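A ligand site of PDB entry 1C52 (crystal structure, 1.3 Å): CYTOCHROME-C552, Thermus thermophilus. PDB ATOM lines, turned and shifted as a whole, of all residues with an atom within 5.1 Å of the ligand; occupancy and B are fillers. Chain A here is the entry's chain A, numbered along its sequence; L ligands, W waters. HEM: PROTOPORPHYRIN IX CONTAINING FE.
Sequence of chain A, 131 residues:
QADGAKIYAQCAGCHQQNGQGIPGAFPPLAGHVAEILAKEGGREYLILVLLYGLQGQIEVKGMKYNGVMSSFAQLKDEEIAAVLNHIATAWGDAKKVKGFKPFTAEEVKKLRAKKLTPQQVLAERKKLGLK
A carbon (CAB) of the ligand is bonded to the side-chain sulfur (SG) of Cys 11 (1.9 Å). SG of Cys 14 is covalently linked to CAC of the ligand (1.9 Å). A ring nitrogen (NE2) of His 15 is bound to an iron atom (FE) of the ligand (2.1 Å). The side-chain sulfur (SD) of Met 69 is bound to an iron atom (FE) of the ligand (2.3 Å). O1D of the ligand lies within hydrogen-bond range of N of Gly 56, 3.3 Å away. O of Gly 56 sits close to O1D of the ligand (2.7 Å). A ring nitrogen (NE2) of His 32 sits at hydrogen-bond distance from an oxygen (O1A) of the ligand (2.7 Å). OH of Tyr 45 is in hydrogen-bond range of O2A of the ligand (2.7 Å). The guanidinium group (NE) of Arg 125 is in salt-bridge range of an oxygen (O2A) of the ligand. The backbone NH of Gly 67 is in hydrogen-bond range of an oxygen (O2D) of the ligand (2.9 Å).
The backbone carbonyl oxygen of Pro 27 lies within hydrogen-bond range of a ring nitrogen (ND1) of His 15, 2.7 Å away. The backbone carbonyl oxygen (O) of Leu 54 sits at hydrogen-bond distance from the backbone NH (N) of Met 69, 2.8 Å away. The backbone NH (N) of Gly 56 lies within hydrogen-bond range of the backbone carbonyl oxygen (O) of Gly 67 (3.5 Å). The backbone NH of Phe 72 lies within hydrogen-bond range of the backbone carbonyl oxygen of Leu 50 (2.7 Å). O of Tyr 65 lies within hydrogen-bond range of N of Ile 58 (2.9 Å). OD1 of Asn 66 sits at hydrogen-bond distance from N of Gln 57, at 3.4 Å.
O of Gln 10 touches CMC of the ligand (3.4 Å). Ala 25 touches the ligand. Phe 26 touches the ligand (CE1 to CAC, 3.7 Å). Pro 27 touches the ligand. Leu 29 touches the ligand. Leu 46 touches the ligand. CG1 of Val 49 touches C2A of the ligand (3.8 Å). CD1 of Leu 50 touches CBB of the ligand (3.7 Å). Leu 54 touches the ligand. Gln 55 touches the ligand. CD1 of Ile 58 touches O1A of the ligand, 3.7 Å away. Val 60 touches the ligand. Tyr 65 touches the ligand (CB to O2D, 3.8 Å). Asn 66 touches the ligand. Val 68 touches the ligand (O to CMD, 3.6 Å). Phe 72 touches the ligand. Hydrophobic or aromatic side chains within 4 Å of the ligand: His 15, Phe 26, Pro 27, Leu 29, His 32, Tyr 45, Leu 46, Val 49, Leu 50, Leu 54, Ile 58, Val 60, Tyr 65, Met 69 and Phe 72. 25 residues have an atom within 4 Å of the ligand: Gln 10, Cys 11, Cys 14, His 15, Ala 25, Phe 26, Pro 27, Leu 29, His 32, Tyr 45, Leu 46, Val 49, Leu 50, Leu 54, Gln 55, Gly 56, Ile 58, Val 60, Tyr 65, Asn 66, Gly 67, Val 68, Met 69, Phe 72 and Arg 125. Along chain A the residues within 4 Å of the ligand span positions 10 to 125.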
ATOM      1  N   ILE A   7       5.843   2.210 -25.987  1.00  0.00           N
ATOM      2  CA  ILE A   7       6.801   1.157 -26.314  1.00  0.00           C
ATOM      3  C   ILE A   7       7.839   1.039 -25.195  1.00  0.00           C
ATOM      4  O   ILE A   7       8.308  -0.071 -24.858  1.00  0.00           O
ATOM      5  CB  ILE A   7       7.458   1.441 -27.647  1.00  0.00           C
ATOM      6  CG1 ILE A   7       6.394   1.401 -28.749  1.00  0.00           C
ATOM      7  CG2 ILE A   7       8.567   0.416 -27.926  1.00  0.00           C
ATOM      8  CD1 ILE A   7       6.777   2.213 -29.959  1.00  0.00           C
ATOM      9  N   TYR A   8       8.165   2.175 -24.578  1.00  0.00           N
ATOM     10  CA  TYR A   8       9.131   2.181 -23.501  1.00  0.00           C
ATOM     11  C   TYR A   8       8.706   1.322 -22.311  1.00  0.00           C
ATOM     12  O   TYR A   8       9.545   0.956 -21.484  1.00  0.00           O
ATOM     13  CB  TYR A   8       9.471   3.612 -23.049  1.00  0.00           C
ATOM     14  CG  TYR A   8      10.610   3.645 -22.053  1.00  0.00           C
ATOM     15  CD1 TYR A   8      11.928   3.451 -22.470  1.00  0.00           C
ATOM     16  CD2 TYR A   8      10.364   3.830 -20.677  1.00  0.00           C
ATOM     17  CE1 TYR A   8      12.982   3.418 -21.542  1.00  0.00           C
ATOM     18  CE2 TYR A   8      11.409   3.796 -19.743  1.00  0.00           C
ATOM     19  CZ  TYR A   8      12.702   3.587 -20.183  1.00  0.00           C
ATOM     20  OH  TYR A   8      13.733   3.523 -19.295  1.00  0.00           O
ATOM     21  N   GLN A  10       8.144  -1.635 -22.331  1.00  0.00           N
ATOM     22  CA  GLN A  10       8.889  -2.882 -22.476  1.00  0.00           C
ATOM     23  C   GLN A  10      10.336  -2.782 -21.962  1.00  0.00           C
ATOM     24  O   GLN A  10      11.004  -3.803 -21.797  1.00  0.00           O
ATOM     25  CB  GLN A  10       8.891  -3.287 -23.956  1.00  0.00           C
ATOM     26  CG  GLN A  10       7.503  -3.538 -24.487  1.00  0.00           C
ATOM     27  CD  GLN A  10       7.522  -3.949 -25.942  1.00  0.00           C
ATOM     28  OE1 GLN A  10       8.371  -4.754 -26.358  1.00  0.00           O
ATOM     29  NE2 GLN A  10       6.601  -3.393 -26.740  1.00  0.00           N
ATOM     30  N   CYS A  11      10.813  -1.563 -21.748  1.00  0.00           N
ATOM     31  CA  CYS A  11      12.177  -1.315 -21.288  1.00  0.00           C
ATOM     32  C   CYS A  11      12.216  -0.895 -19.834  1.00  0.00           C
ATOM     33  O   CYS A  11      13.255  -1.027 -19.182  1.00  0.00           O
ATOM     34  CB  CYS A  11      12.791  -0.145 -22.062  1.00  0.00           C
ATOM     35  SG  CYS A  11      12.288   0.045 -23.776  1.00  0.00           S
ATOM     36  N   CYS A  14      13.654  -2.687 -16.531  1.00  0.00           N
ATOM     37  CA  CYS A  14      15.091  -2.670 -16.406  1.00  0.00           C
ATOM     38  C   CYS A  14      15.679  -1.249 -16.272  1.00  0.00           C
ATOM     39  O   CYS A  14      16.323  -0.924 -15.276  1.00  0.00           O
ATOM     40  CB  CYS A  14      15.714  -3.361 -17.610  1.00  0.00           C
ATOM     41  SG  CYS A  14      15.235  -5.098 -17.671  1.00  0.00           S
ATOM     42  N   HIS A  15      15.440  -0.406 -17.278  1.00  0.00           N
ATOM     43  CA  HIS A  15      15.993   0.940 -17.263  1.00  0.00           C
ATOM     44  C   HIS A  15      15.208   1.978 -16.436  1.00  0.00           C
ATOM     45  O   HIS A  15      15.733   3.086 -16.195  1.00  0.00           O
ATOM     46  CB  HIS A  15      16.183   1.428 -18.701  1.00  0.00           C
ATOM     47  CG  HIS A  15      17.148   0.591 -19.471  1.00  0.00           C
ATOM     48  ND1 HIS A  15      18.505   0.636 -19.243  1.00  0.00           N
ATOM     49  CD2 HIS A  15      16.965  -0.304 -20.471  1.00  0.00           C
ATOM     50  CE1 HIS A  15      19.119  -0.206 -20.064  1.00  0.00           C
ATOM     51  NE2 HIS A  15      18.208  -0.778 -20.826  1.00  0.00           N
ATOM     52  N   ALA A  25      23.170  -3.440 -12.285  1.00  0.00           N
ATOM     53  CA  ALA A  25      22.269  -4.295 -13.022  1.00  0.00           C
ATOM     54  C   ALA A  25      21.928  -3.783 -14.411  1.00  0.00           C
ATOM     55  O   ALA A  25      22.292  -4.393 -15.422  1.00  0.00           O
ATOM     56  CB  ALA A  25      20.991  -4.552 -12.216  1.00  0.00           C
ATOM     57  N   PHE A  26      21.227  -2.642 -14.473  1.00  0.00           N
ATOM     58  CA  PHE A  26      20.775  -2.073 -15.743  1.00  0.00           C
ATOM     59  C   PHE A  26      21.247  -0.645 -15.813  1.00  0.00           C
ATOM     60  O   PHE A  26      20.948   0.155 -14.916  1.00  0.00           O
ATOM     61  CB  PHE A  26      19.253  -2.174 -15.814  1.00  0.00           C
ATOM     62  CG  PHE A  26      18.732  -3.550 -15.483  1.00  0.00           C
ATOM     63  CD1 PHE A  26      19.119  -4.655 -16.266  1.00  0.00           C
ATOM     64  CD2 PHE A  26      17.891  -3.763 -14.403  1.00  0.00           C
ATOM     65  CE1 PHE A  26      18.670  -5.965 -15.957  1.00  0.00           C
ATOM     66  CE2 PHE A  26      17.432  -5.057 -14.071  1.00  0.00           C
ATOM     67  CZ  PHE A  26      17.835  -6.160 -14.864  1.00  0.00           C
ATOM     68  N   PRO A  27      21.983  -0.292 -16.873  1.00  0.00           N
ATOM     69  CA  PRO A  27      22.466   1.074 -16.940  1.00  0.00           C
ATOM     70  C   PRO A  27      21.418   2.166 -17.129  1.00  0.00           C
ATOM     71  O   PRO A  27      20.344   1.936 -17.679  1.00  0.00           O
ATOM     72  CB  PRO A  27      23.484   1.042 -18.082  1.00  0.00           C
ATOM     73  CG  PRO A  27      22.914   0.029 -18.995  1.00  0.00           C
ATOM     74  CD  PRO A  27      22.406  -1.056 -18.063  1.00  0.00           C
ATOM     75  N   LEU A  29      19.702   5.494 -18.683  1.00  0.00           N
ATOM     76  CA  LEU A  29      19.584   6.034 -20.024  1.00  0.00           C
ATOM     77  C   LEU A  29      19.499   7.570 -19.868  1.00  0.00           C
ATOM     78  O   LEU A  29      20.062   8.290 -20.690  1.00  0.00           O
ATOM     79  CB  LEU A  29      18.338   5.488 -20.753  1.00  0.00           C
ATOM     80  CG  LEU A  29      18.330   3.972 -20.987  1.00  0.00           C
ATOM     81  CD1 LEU A  29      17.052   3.556 -21.699  1.00  0.00           C
ATOM     82  CD2 LEU A  29      19.580   3.569 -21.782  1.00  0.00           C
ATOM     83  N   HIS A  32      22.769   9.773 -19.906  1.00  0.00           N
ATOM     84  CA  HIS A  32      23.690   8.954 -20.665  1.00  0.00           C
ATOM     85  C   HIS A  32      23.459   8.971 -22.178  1.00  0.00           C
ATOM     86  O   HIS A  32      24.426   8.988 -22.956  1.00  0.00           O
ATOM     87  CB  HIS A  32      23.597   7.553 -20.070  1.00  0.00           C
ATOM     88  CG  HIS A  32      24.512   6.565 -20.715  1.00  0.00           C
ATOM     89  ND1 HIS A  32      25.859   6.814 -20.921  1.00  0.00           N
ATOM     90  CD2 HIS A  32      24.286   5.323 -21.191  1.00  0.00           C
ATOM     91  CE1 HIS A  32      26.412   5.759 -21.485  1.00  0.00           C
ATOM     92  NE2 HIS A  32      25.476   4.844 -21.660  1.00  0.00           N
ATOM     93  N   ILE A  36      26.161   9.596 -25.463  1.00  0.00           N
ATOM     94  CA  ILE A  36      26.385   8.722 -26.612  1.00  0.00           C
ATOM     95  C   ILE A  36      26.133   9.459 -27.910  1.00  0.00           C
ATOM     96  O   ILE A  36      26.908   9.356 -28.869  1.00  0.00           O
ATOM     97  CB  ILE A  36      25.482   7.469 -26.528  1.00  0.00           C
ATOM     98  CG1 ILE A  36      25.949   6.576 -25.360  1.00  0.00           C
ATOM     99  CG2 ILE A  36      25.504   6.711 -27.857  1.00  0.00           C
ATOM    100  CD1 ILE A  36      24.956   5.485 -24.997  1.00  0.00           C
ATOM    101  N   TYR A  45      24.851   3.593 -33.297  1.00  0.00           N
ATOM    102  CA  TYR A  45      25.075   2.653 -32.228  1.00  0.00           C
ATOM    103  C   TYR A  45      23.801   2.344 -31.463  1.00  0.00           C
ATOM    104  O   TYR A  45      23.488   1.175 -31.193  1.00  0.00           O
ATOM    105  CB  TYR A  45      26.129   3.177 -31.267  1.00  0.00           C
ATOM    106  CG  TYR A  45      26.205   2.350 -30.014  1.00  0.00           C
ATOM    107  CD1 TYR A  45      26.700   1.050 -30.056  1.00  0.00           C
ATOM    108  CD2 TYR A  45      25.735   2.850 -28.790  1.00  0.00           C
ATOM    109  CE1 TYR A  45      26.720   0.254 -28.932  1.00  0.00           C
ATOM    110  CE2 TYR A  45      25.747   2.062 -27.658  1.00  0.00           C
ATOM    111  CZ  TYR A  45      26.240   0.751 -27.739  1.00  0.00           C
ATOM    112  OH  TYR A  45      26.251  -0.068 -26.652  1.00  0.00           O
ATOM    113  N   LEU A  46      23.058   3.375 -31.094  1.00  0.00           N
ATOM    114  CA  LEU A  46      21.815   3.183 -30.347  1.00  0.00           C
ATOM    115  C   LEU A  46      20.821   2.328 -31.131  1.00  0.00           C
ATOM    116  O   LEU A  46      20.099   1.511 -30.545  1.00  0.00           O
ATOM    117  CB  LEU A  46      21.204   4.541 -29.981  1.00  0.00           C
ATOM    118  CG  LEU A  46      22.070   5.267 -28.948  1.00  0.00           C
ATOM    119  CD1 LEU A  46      21.634   6.713 -28.789  1.00  0.00           C
ATOM    120  CD2 LEU A  46      21.987   4.517 -27.626  1.00  0.00           C
ATOM    121  N   VAL A  49      21.964  -1.310 -30.947  1.00  0.00           N
ATOM    122  CA  VAL A  49      21.603  -1.950 -29.687  1.00  0.00           C
ATOM    123  C   VAL A  49      20.173  -2.474 -29.751  1.00  0.00           C
ATOM    124  O   VAL A  49      19.888  -3.604 -29.342  1.00  0.00           O
ATOM    125  CB  VAL A  49      21.714  -0.968 -28.488  1.00  0.00           C
ATOM    126  CG1 VAL A  49      21.156  -1.618 -27.214  1.00  0.00           C
ATOM    127  CG2 VAL A  49      23.175  -0.583 -28.266  1.00  0.00           C
ATOM    128  N   LEU A  50      19.262  -1.653 -30.279  1.00  0.00           N
ATOM    129  CA  LEU A  50      17.874  -2.056 -30.382  1.00  0.00           C
ATOM    130  C   LEU A  50      17.634  -3.188 -31.373  1.00  0.00           C
ATOM    131  O   LEU A  50      16.811  -4.065 -31.143  1.00  0.00           O
ATOM    132  CB  LEU A  50      17.001  -0.840 -30.716  1.00  0.00           C
ATOM    133  CG  LEU A  50      16.541  -0.038 -29.464  1.00  0.00           C
ATOM    134  CD1 LEU A  50      15.416  -0.774 -28.770  1.00  0.00           C
ATOM    135  CD2 LEU A  50      17.670   0.201 -28.474  1.00  0.00           C
ATOM    136  N   LEU A  54      23.018  -6.297 -26.920  1.00  0.00           N
ATOM    137  CA  LEU A  54      24.343  -5.908 -26.448  1.00  0.00           C
ATOM    138  C   LEU A  54      24.745  -6.831 -25.328  1.00  0.00           C
ATOM    139  O   LEU A  54      23.900  -7.234 -24.529  1.00  0.00           O
ATOM    140  CB  LEU A  54      24.302  -4.453 -25.905  1.00  0.00           C
ATOM    141  CG  LEU A  54      25.572  -3.857 -25.257  1.00  0.00           C
ATOM    142  CD1 LEU A  54      26.685  -3.696 -26.307  1.00  0.00           C
ATOM    143  CD2 LEU A  54      25.236  -2.485 -24.609  1.00  0.00           C
ATOM    144  N   GLN A  55      26.030  -7.169 -25.254  1.00  0.00           N
ATOM    145  CA  GLN A  55      26.551  -8.002 -24.173  1.00  0.00           C
ATOM    146  C   GLN A  55      27.992  -7.625 -23.964  1.00  0.00           C
ATOM    147  O   GLN A  55      28.660  -7.209 -24.896  1.00  0.00           O
ATOM    148  CB  GLN A  55      26.455  -9.493 -24.514  1.00  0.00           C
ATOM    149  CG  GLN A  55      25.016 -10.020 -24.610  1.00  0.00           C
ATOM    150  CD  GLN A  55      24.963 -11.474 -25.022  1.00  0.00           C
ATOM    151  OE1 GLN A  55      25.911 -12.228 -24.781  1.00  0.00           O
ATOM    152  NE2 GLN A  55      23.839 -11.885 -25.631  1.00  0.00           N
ATOM    153  N   GLY A  56      28.481  -7.761 -22.742  1.00  0.00           N
ATOM    154  CA  GLY A  56      29.870  -7.433 -22.495  1.00  0.00           C
ATOM    155  C   GLY A  56      30.015  -6.370 -21.426  1.00  0.00           C
ATOM    156  O   GLY A  56      29.048  -5.730 -21.041  1.00  0.00           O
ATOM    157  N   GLN A  57      31.228  -6.186 -20.949  1.00  0.00           N
ATOM    158  CA  GLN A  57      31.474  -5.208 -19.912  1.00  0.00           C
ATOM    159  C   GLN A  57      31.490  -3.784 -20.471  1.00  0.00           C
ATOM    160  O   GLN A  57      32.153  -3.472 -21.487  1.00  0.00           O
ATOM    161  CB  GLN A  57      32.786  -5.515 -19.184  1.00  0.00           C
ATOM    162  CG  GLN A  57      32.952  -4.757 -17.865  1.00  0.00           C
ATOM    163  N   ILE A  58      30.734  -2.912 -19.817  1.00  0.00           N
ATOM    164  CA  ILE A  58      30.682  -1.509 -20.194  1.00  0.00           C
ATOM    165  C   ILE A  58      30.711  -0.701 -18.904  1.00  0.00           C
ATOM    166  O   ILE A  58      30.468  -1.233 -17.803  1.00  0.00           O
ATOM    167  CB  ILE A  58      29.377  -1.126 -20.984  1.00  0.00           C
ATOM    168  CG1 ILE A  58      28.123  -1.400 -20.148  1.00  0.00           C
ATOM    169  CG2 ILE A  58      29.309  -1.909 -22.291  1.00  0.00           C
ATOM    170  CD1 ILE A  58      26.838  -0.932 -20.819  1.00  0.00           C
ATOM    171  N   VAL A  60      29.213   3.010 -17.359  1.00  0.00           N
ATOM    172  CA  VAL A  60      28.260   4.065 -17.612  1.00  0.00           C
ATOM    173  C   VAL A  60      28.228   4.897 -16.335  1.00  0.00           C
ATOM    174  O   VAL A  60      28.002   4.358 -15.248  1.00  0.00           O
ATOM    175  CB  VAL A  60      26.855   3.496 -17.882  1.00  0.00           C
ATOM    176  CG1 VAL A  60      25.827   4.634 -17.960  1.00  0.00           C
ATOM    177  CG2 VAL A  60      26.848   2.697 -19.210  1.00  0.00           C
ATOM    178  N   TYR A  65      28.968  -2.424 -15.669  1.00  0.00           N
ATOM    179  CA  TYR A  65      27.860  -3.328 -15.969  1.00  0.00           C
ATOM    180  C   TYR A  65      28.442  -4.425 -16.839  1.00  0.00           C
ATOM    181  O   TYR A  65      29.265  -4.176 -17.723  1.00  0.00           O
ATOM    182  CB  TYR A  65      26.758  -2.620 -16.750  1.00  0.00           C
ATOM    183  CG  TYR A  65      26.146  -1.488 -15.987  1.00  0.00           C
ATOM    184  CD1 TYR A  65      26.710  -0.205 -16.008  1.00  0.00           C
ATOM    185  CD2 TYR A  65      25.015  -1.713 -15.191  1.00  0.00           C
ATOM    186  CE1 TYR A  65      26.184   0.831 -15.230  1.00  0.00           C
ATOM    187  CE2 TYR A  65      24.476  -0.686 -14.417  1.00  0.00           C
ATOM    188  CZ  TYR A  65      25.067   0.585 -14.436  1.00  0.00           C
ATOM    189  OH  TYR A  65      24.545   1.587 -13.643  1.00  0.00           O
ATOM    190  N   ASN A  66      28.042  -5.651 -16.584  1.00  0.00           N
ATOM    191  CA  ASN A  66      28.494  -6.756 -17.414  1.00  0.00           C
ATOM    192  C   ASN A  66      27.282  -7.634 -17.557  1.00  0.00           C
ATOM    193  O   ASN A  66      27.191  -8.697 -16.957  1.00  0.00           O
ATOM    194  CB  ASN A  66      29.641  -7.530 -16.743  1.00  0.00           C
ATOM    195  CG  ASN A  66      30.312  -8.528 -17.692  1.00  0.00           C
ATOM    196  OD1 ASN A  66      29.979  -8.597 -18.875  1.00  0.00           O
ATOM    197  ND2 ASN A  66      31.253  -9.298 -17.161  1.00  0.00           N
ATOM    198  N   GLY A  67      26.323  -7.158 -18.321  1.00  0.00           N
ATOM    199  CA  GLY A  67      25.095  -7.895 -18.494  1.00  0.00           C
ATOM    200  C   GLY A  67      24.754  -8.149 -19.942  1.00  0.00           C
ATOM    201  O   GLY A  67      25.606  -8.121 -20.849  1.00  0.00           O
ATOM    202  N   VAL A  68      23.484  -8.453 -20.169  1.00  0.00           N
ATOM    203  CA  VAL A  68      23.021  -8.743 -21.500  1.00  0.00           C
ATOM    204  C   VAL A  68      21.711  -8.057 -21.786  1.00  0.00           C
ATOM    205  O   VAL A  68      20.822  -7.981 -20.927  1.00  0.00           O
ATOM    206  CB  VAL A  68      22.817 -10.281 -21.723  1.00  0.00           C
ATOM    207  CG1 VAL A  68      24.022 -11.046 -21.269  1.00  0.00           C
ATOM    208  CG2 VAL A  68      21.645 -10.781 -20.976  1.00  0.00           C
ATOM    209  N   MET A  69      21.590  -7.538 -22.992  1.00  0.00           N
ATOM    210  CA  MET A  69      20.349  -6.954 -23.414  1.00  0.00           C
ATOM    211  C   MET A  69      19.935  -7.658 -24.692  1.00  0.00           C
ATOM    212  O   MET A  69      20.741  -7.776 -25.627  1.00  0.00           O
ATOM    213  CB  MET A  69      20.465  -5.489 -23.710  1.00  0.00           C
ATOM    214  CG  MET A  69      19.098  -4.985 -24.137  1.00  0.00           C
ATOM    215  SD  MET A  69      19.092  -3.251 -24.304  1.00  0.00           S
ATOM    216  CE  MET A  69      18.018  -2.990 -25.640  1.00  0.00           C
ATOM    217  N   PHE A  72      15.561  -6.083 -29.965  1.00  0.00           N
ATOM    218  CA  PHE A  72      14.134  -5.750 -30.051  1.00  0.00           C
ATOM    219  C   PHE A  72      13.798  -5.597 -31.529  1.00  0.00           C
ATOM    220  O   PHE A  72      12.963  -4.789 -31.914  1.00  0.00           O
ATOM    221  CB  PHE A  72      13.810  -4.458 -29.281  1.00  0.00           C
ATOM    222  CG  PHE A  72      13.663  -4.676 -27.810  1.00  0.00           C
ATOM    223  CD1 PHE A  72      14.786  -4.829 -26.985  1.00  0.00           C
ATOM    224  CD2 PHE A  72      12.378  -4.754 -27.243  1.00  0.00           C
ATOM    225  CE1 PHE A  72      14.651  -5.043 -25.622  1.00  0.00           C
ATOM    226  CE2 PHE A  72      12.224  -4.973 -25.855  1.00  0.00           C
ATOM    227  CZ  PHE A  72      13.372  -5.123 -25.047  1.00  0.00           C
ATOM    228  N   LEU A  75      10.295  -5.325 -33.150  1.00  0.00           N
ATOM    229  CA  LEU A  75       9.523  -4.078 -33.223  1.00  0.00           C
ATOM    230  C   LEU A  75       9.608  -3.528 -34.657  1.00  0.00           C
ATOM    231  O   LEU A  75      10.571  -3.792 -35.376  1.00  0.00           O
ATOM    232  CB  LEU A  75      10.086  -3.026 -32.257  1.00  0.00           C
ATOM    233  CG  LEU A  75      10.024  -3.256 -30.737  1.00  0.00           C
ATOM    234  CD1 LEU A  75      10.733  -2.120 -30.007  1.00  0.00           C
ATOM    235  CD2 LEU A  75       8.595  -3.325 -30.291  1.00  0.00           C
ATOM    236  N   VAL A  83      10.744   4.690 -29.792  1.00  0.00           N
ATOM    237  CA  VAL A  83      11.274   4.475 -28.455  1.00  0.00           C
ATOM    238  C   VAL A  83      12.647   5.125 -28.269  1.00  0.00           C
ATOM    239  O   VAL A  83      12.992   5.573 -27.167  1.00  0.00           O
ATOM    240  CB  VAL A  83      11.265   2.963 -28.048  1.00  0.00           C
ATOM    241  CG1 VAL A  83      12.417   2.191 -28.710  1.00  0.00           C
ATOM    242  CG2 VAL A  83      11.387   2.841 -26.521  1.00  0.00           C
ATOM    243  N   LEU A  84      13.452   5.176 -29.313  1.00  0.00           N
ATOM    244  CA  LEU A  84      14.747   5.829 -29.221  1.00  0.00           C
ATOM    245  C   LEU A  84      14.529   7.342 -29.050  1.00  0.00           C
ATOM    246  O   LEU A  84      15.230   7.999 -28.292  1.00  0.00           O
ATOM    247  CB  LEU A  84      15.576   5.525 -30.467  1.00  0.00           C
ATOM    248  CG  LEU A  84      16.135   4.091 -30.462  1.00  0.00           C
ATOM    249  CD1 LEU A  84      16.815   3.790 -31.801  1.00  0.00           C
ATOM    250  CD2 LEU A  84      17.097   3.900 -29.292  1.00  0.00           C
ATOM    251  N   ILE A  87      13.643   7.775 -25.322  1.00  0.00           N
ATOM    252  CA  ILE A  87      14.754   7.817 -24.366  1.00  0.00           C
ATOM    253  C   ILE A  87      15.645   9.043 -24.599  1.00  0.00           C
ATOM    254  O   ILE A  87      16.343   9.469 -23.680  1.00  0.00           O
ATOM    255  CB  ILE A  87      15.597   6.510 -24.346  1.00  0.00           C
ATOM    256  CG1 ILE A  87      16.358   6.308 -25.670  1.00  0.00           C
ATOM    257  CG2 ILE A  87      14.682   5.358 -24.079  1.00  0.00           C
ATOM    258  CD1 ILE A  87      17.366   5.143 -25.609  1.00  0.00           C
ATOM    259  N   ARG A 125      30.479  -0.057 -29.927  1.00  0.00           N
ATOM    260  CA  ARG A 125      30.466   0.867 -28.780  1.00  0.00           C
ATOM    261  C   ARG A 125      31.872   1.332 -28.461  1.00  0.00           C
ATOM    262  O   ARG A 125      32.097   2.514 -28.212  1.00  0.00           O
ATOM    263  CB  ARG A 125      29.899   0.164 -27.549  1.00  0.00           C
ATOM    264  CG  ARG A 125      29.598   1.099 -26.392  1.00  0.00           C
ATOM    265  CD  ARG A 125      29.095   0.272 -25.201  1.00  0.00           C
ATOM    266  NE  ARG A 125      28.542   1.120 -24.147  1.00  0.00           N
ATOM    267  CZ  ARG A 125      29.272   1.750 -23.227  1.00  0.00           C
ATOM    268  NH1 ARG A 125      30.608   1.653 -23.221  1.00  0.00           N
ATOM    269  NH2 ARG A 125      28.656   2.487 -22.306  1.00  0.00           N
HETATM  270  CHA HEM L   1      21.893  -1.566 -22.498  1.00  0.00           C
HETATM  271  CHB HEM L   1      18.032   0.690 -24.336  1.00  0.00           C
HETATM  272  CHC HEM L   1      15.251  -2.929 -22.783  1.00  0.00           C
HETATM  273  CHD HEM L   1      18.910  -4.449 -20.044  1.00  0.00           C
HETATM  274  C1A HEM L   1      21.084  -0.671 -23.219  1.00  0.00           C
HETATM  275  C2A HEM L   1      21.584   0.444 -24.013  1.00  0.00           C
HETATM  276  C3A HEM L   1      20.493   1.103 -24.501  1.00  0.00           C
HETATM  277  C4A HEM L   1      19.331   0.392 -24.000  1.00  0.00           C
HETATM  278  CMA HEM L   1      20.436   2.322 -25.409  1.00  0.00           C
HETATM  279  CAA HEM L   1      23.053   0.749 -24.243  1.00  0.00           C
HETATM  280  CBA HEM L   1      23.702   1.495 -23.112  1.00  0.00           C
HETATM  281  CGA HEM L   1      25.191   1.664 -23.289  1.00  0.00           C
HETATM  282  O1A HEM L   1      25.823   2.288 -22.425  1.00  0.00           O
HETATM  283  O2A HEM L   1      25.767   1.172 -24.286  1.00  0.00           O
HETATM  284  C1B HEM L   1      16.925  -0.093 -24.056  1.00  0.00           C
HETATM  285  C2B HEM L   1      15.612   0.138 -24.587  1.00  0.00           C
HETATM  286  C3B HEM L   1      14.808  -0.914 -24.225  1.00  0.00           C
HETATM  287  C4B HEM L   1      15.708  -1.775 -23.435  1.00  0.00           C
HETATM  288  CMB HEM L   1      15.222   1.405 -25.382  1.00  0.00           C
HETATM  289  CAB HEM L   1      13.440  -1.196 -24.539  1.00  0.00           C
HETATM  290  CBB HEM L   1      13.029  -1.245 -25.937  1.00  0.00           C
HETATM  291  C1C HEM L   1      16.052  -3.653 -21.876  1.00  0.00           C
HETATM  292  C2C HEM L   1      15.477  -4.625 -20.982  1.00  0.00           C
HETATM  293  C3C HEM L   1      16.493  -4.997 -20.095  1.00  0.00           C
HETATM  294  C4C HEM L   1      17.654  -4.259 -20.538  1.00  0.00           C
HETATM  295  CMC HEM L   1      14.043  -5.174 -20.986  1.00  0.00           C
HETATM  296  CAC HEM L   1      16.453  -5.796 -18.916  1.00  0.00           C
HETATM  297  CBC HEM L   1      16.093  -7.202 -18.946  1.00  0.00           C
HETATM  298  C1D HEM L   1      20.051  -3.804 -20.484  1.00  0.00           C
HETATM  299  C2D HEM L   1      21.378  -4.132 -20.061  1.00  0.00           C
HETATM  300  C3D HEM L   1      22.222  -3.367 -20.784  1.00  0.00           C
HETATM  301  C4D HEM L   1      21.397  -2.559 -21.654  1.00  0.00           C
HETATM  302  CMD HEM L   1      21.754  -5.119 -18.975  1.00  0.00           C
HETATM  303  CAD HEM L   1      23.755  -3.395 -20.689  1.00  0.00           C
HETATM  304  CBD HEM L   1      24.339  -4.583 -21.432  1.00  0.00           C
HETATM  305  CGD HEM L   1      25.784  -4.851 -21.055  1.00  0.00           C
HETATM  306  O1D HEM L   1      26.607  -5.159 -21.972  1.00  0.00           O
HETATM  307  O2D HEM L   1      26.101  -4.754 -19.854  1.00  0.00           O
HETATM  308  NA  HEM L   1      19.693  -0.692 -23.241  1.00  0.00           N
HETATM  309  NB  HEM L   1      16.956  -1.261 -23.318  1.00  0.00           N
HETATM  310  NC  HEM L   1      17.350  -3.406 -21.583  1.00  0.00           N
HETATM  311  ND  HEM L   1      20.088  -2.845 -21.471  1.00  0.00           N
HETATM  312 FE   HEM L   1      18.524  -2.051 -22.427  1.00  0.00          FE
HETATM  313  O   HOH W   1      11.909  -3.986 -18.940  1.00  0.00           O
HETATM  314  O   HOH W   2      16.870  -7.271 -22.646  1.00  0.00           O
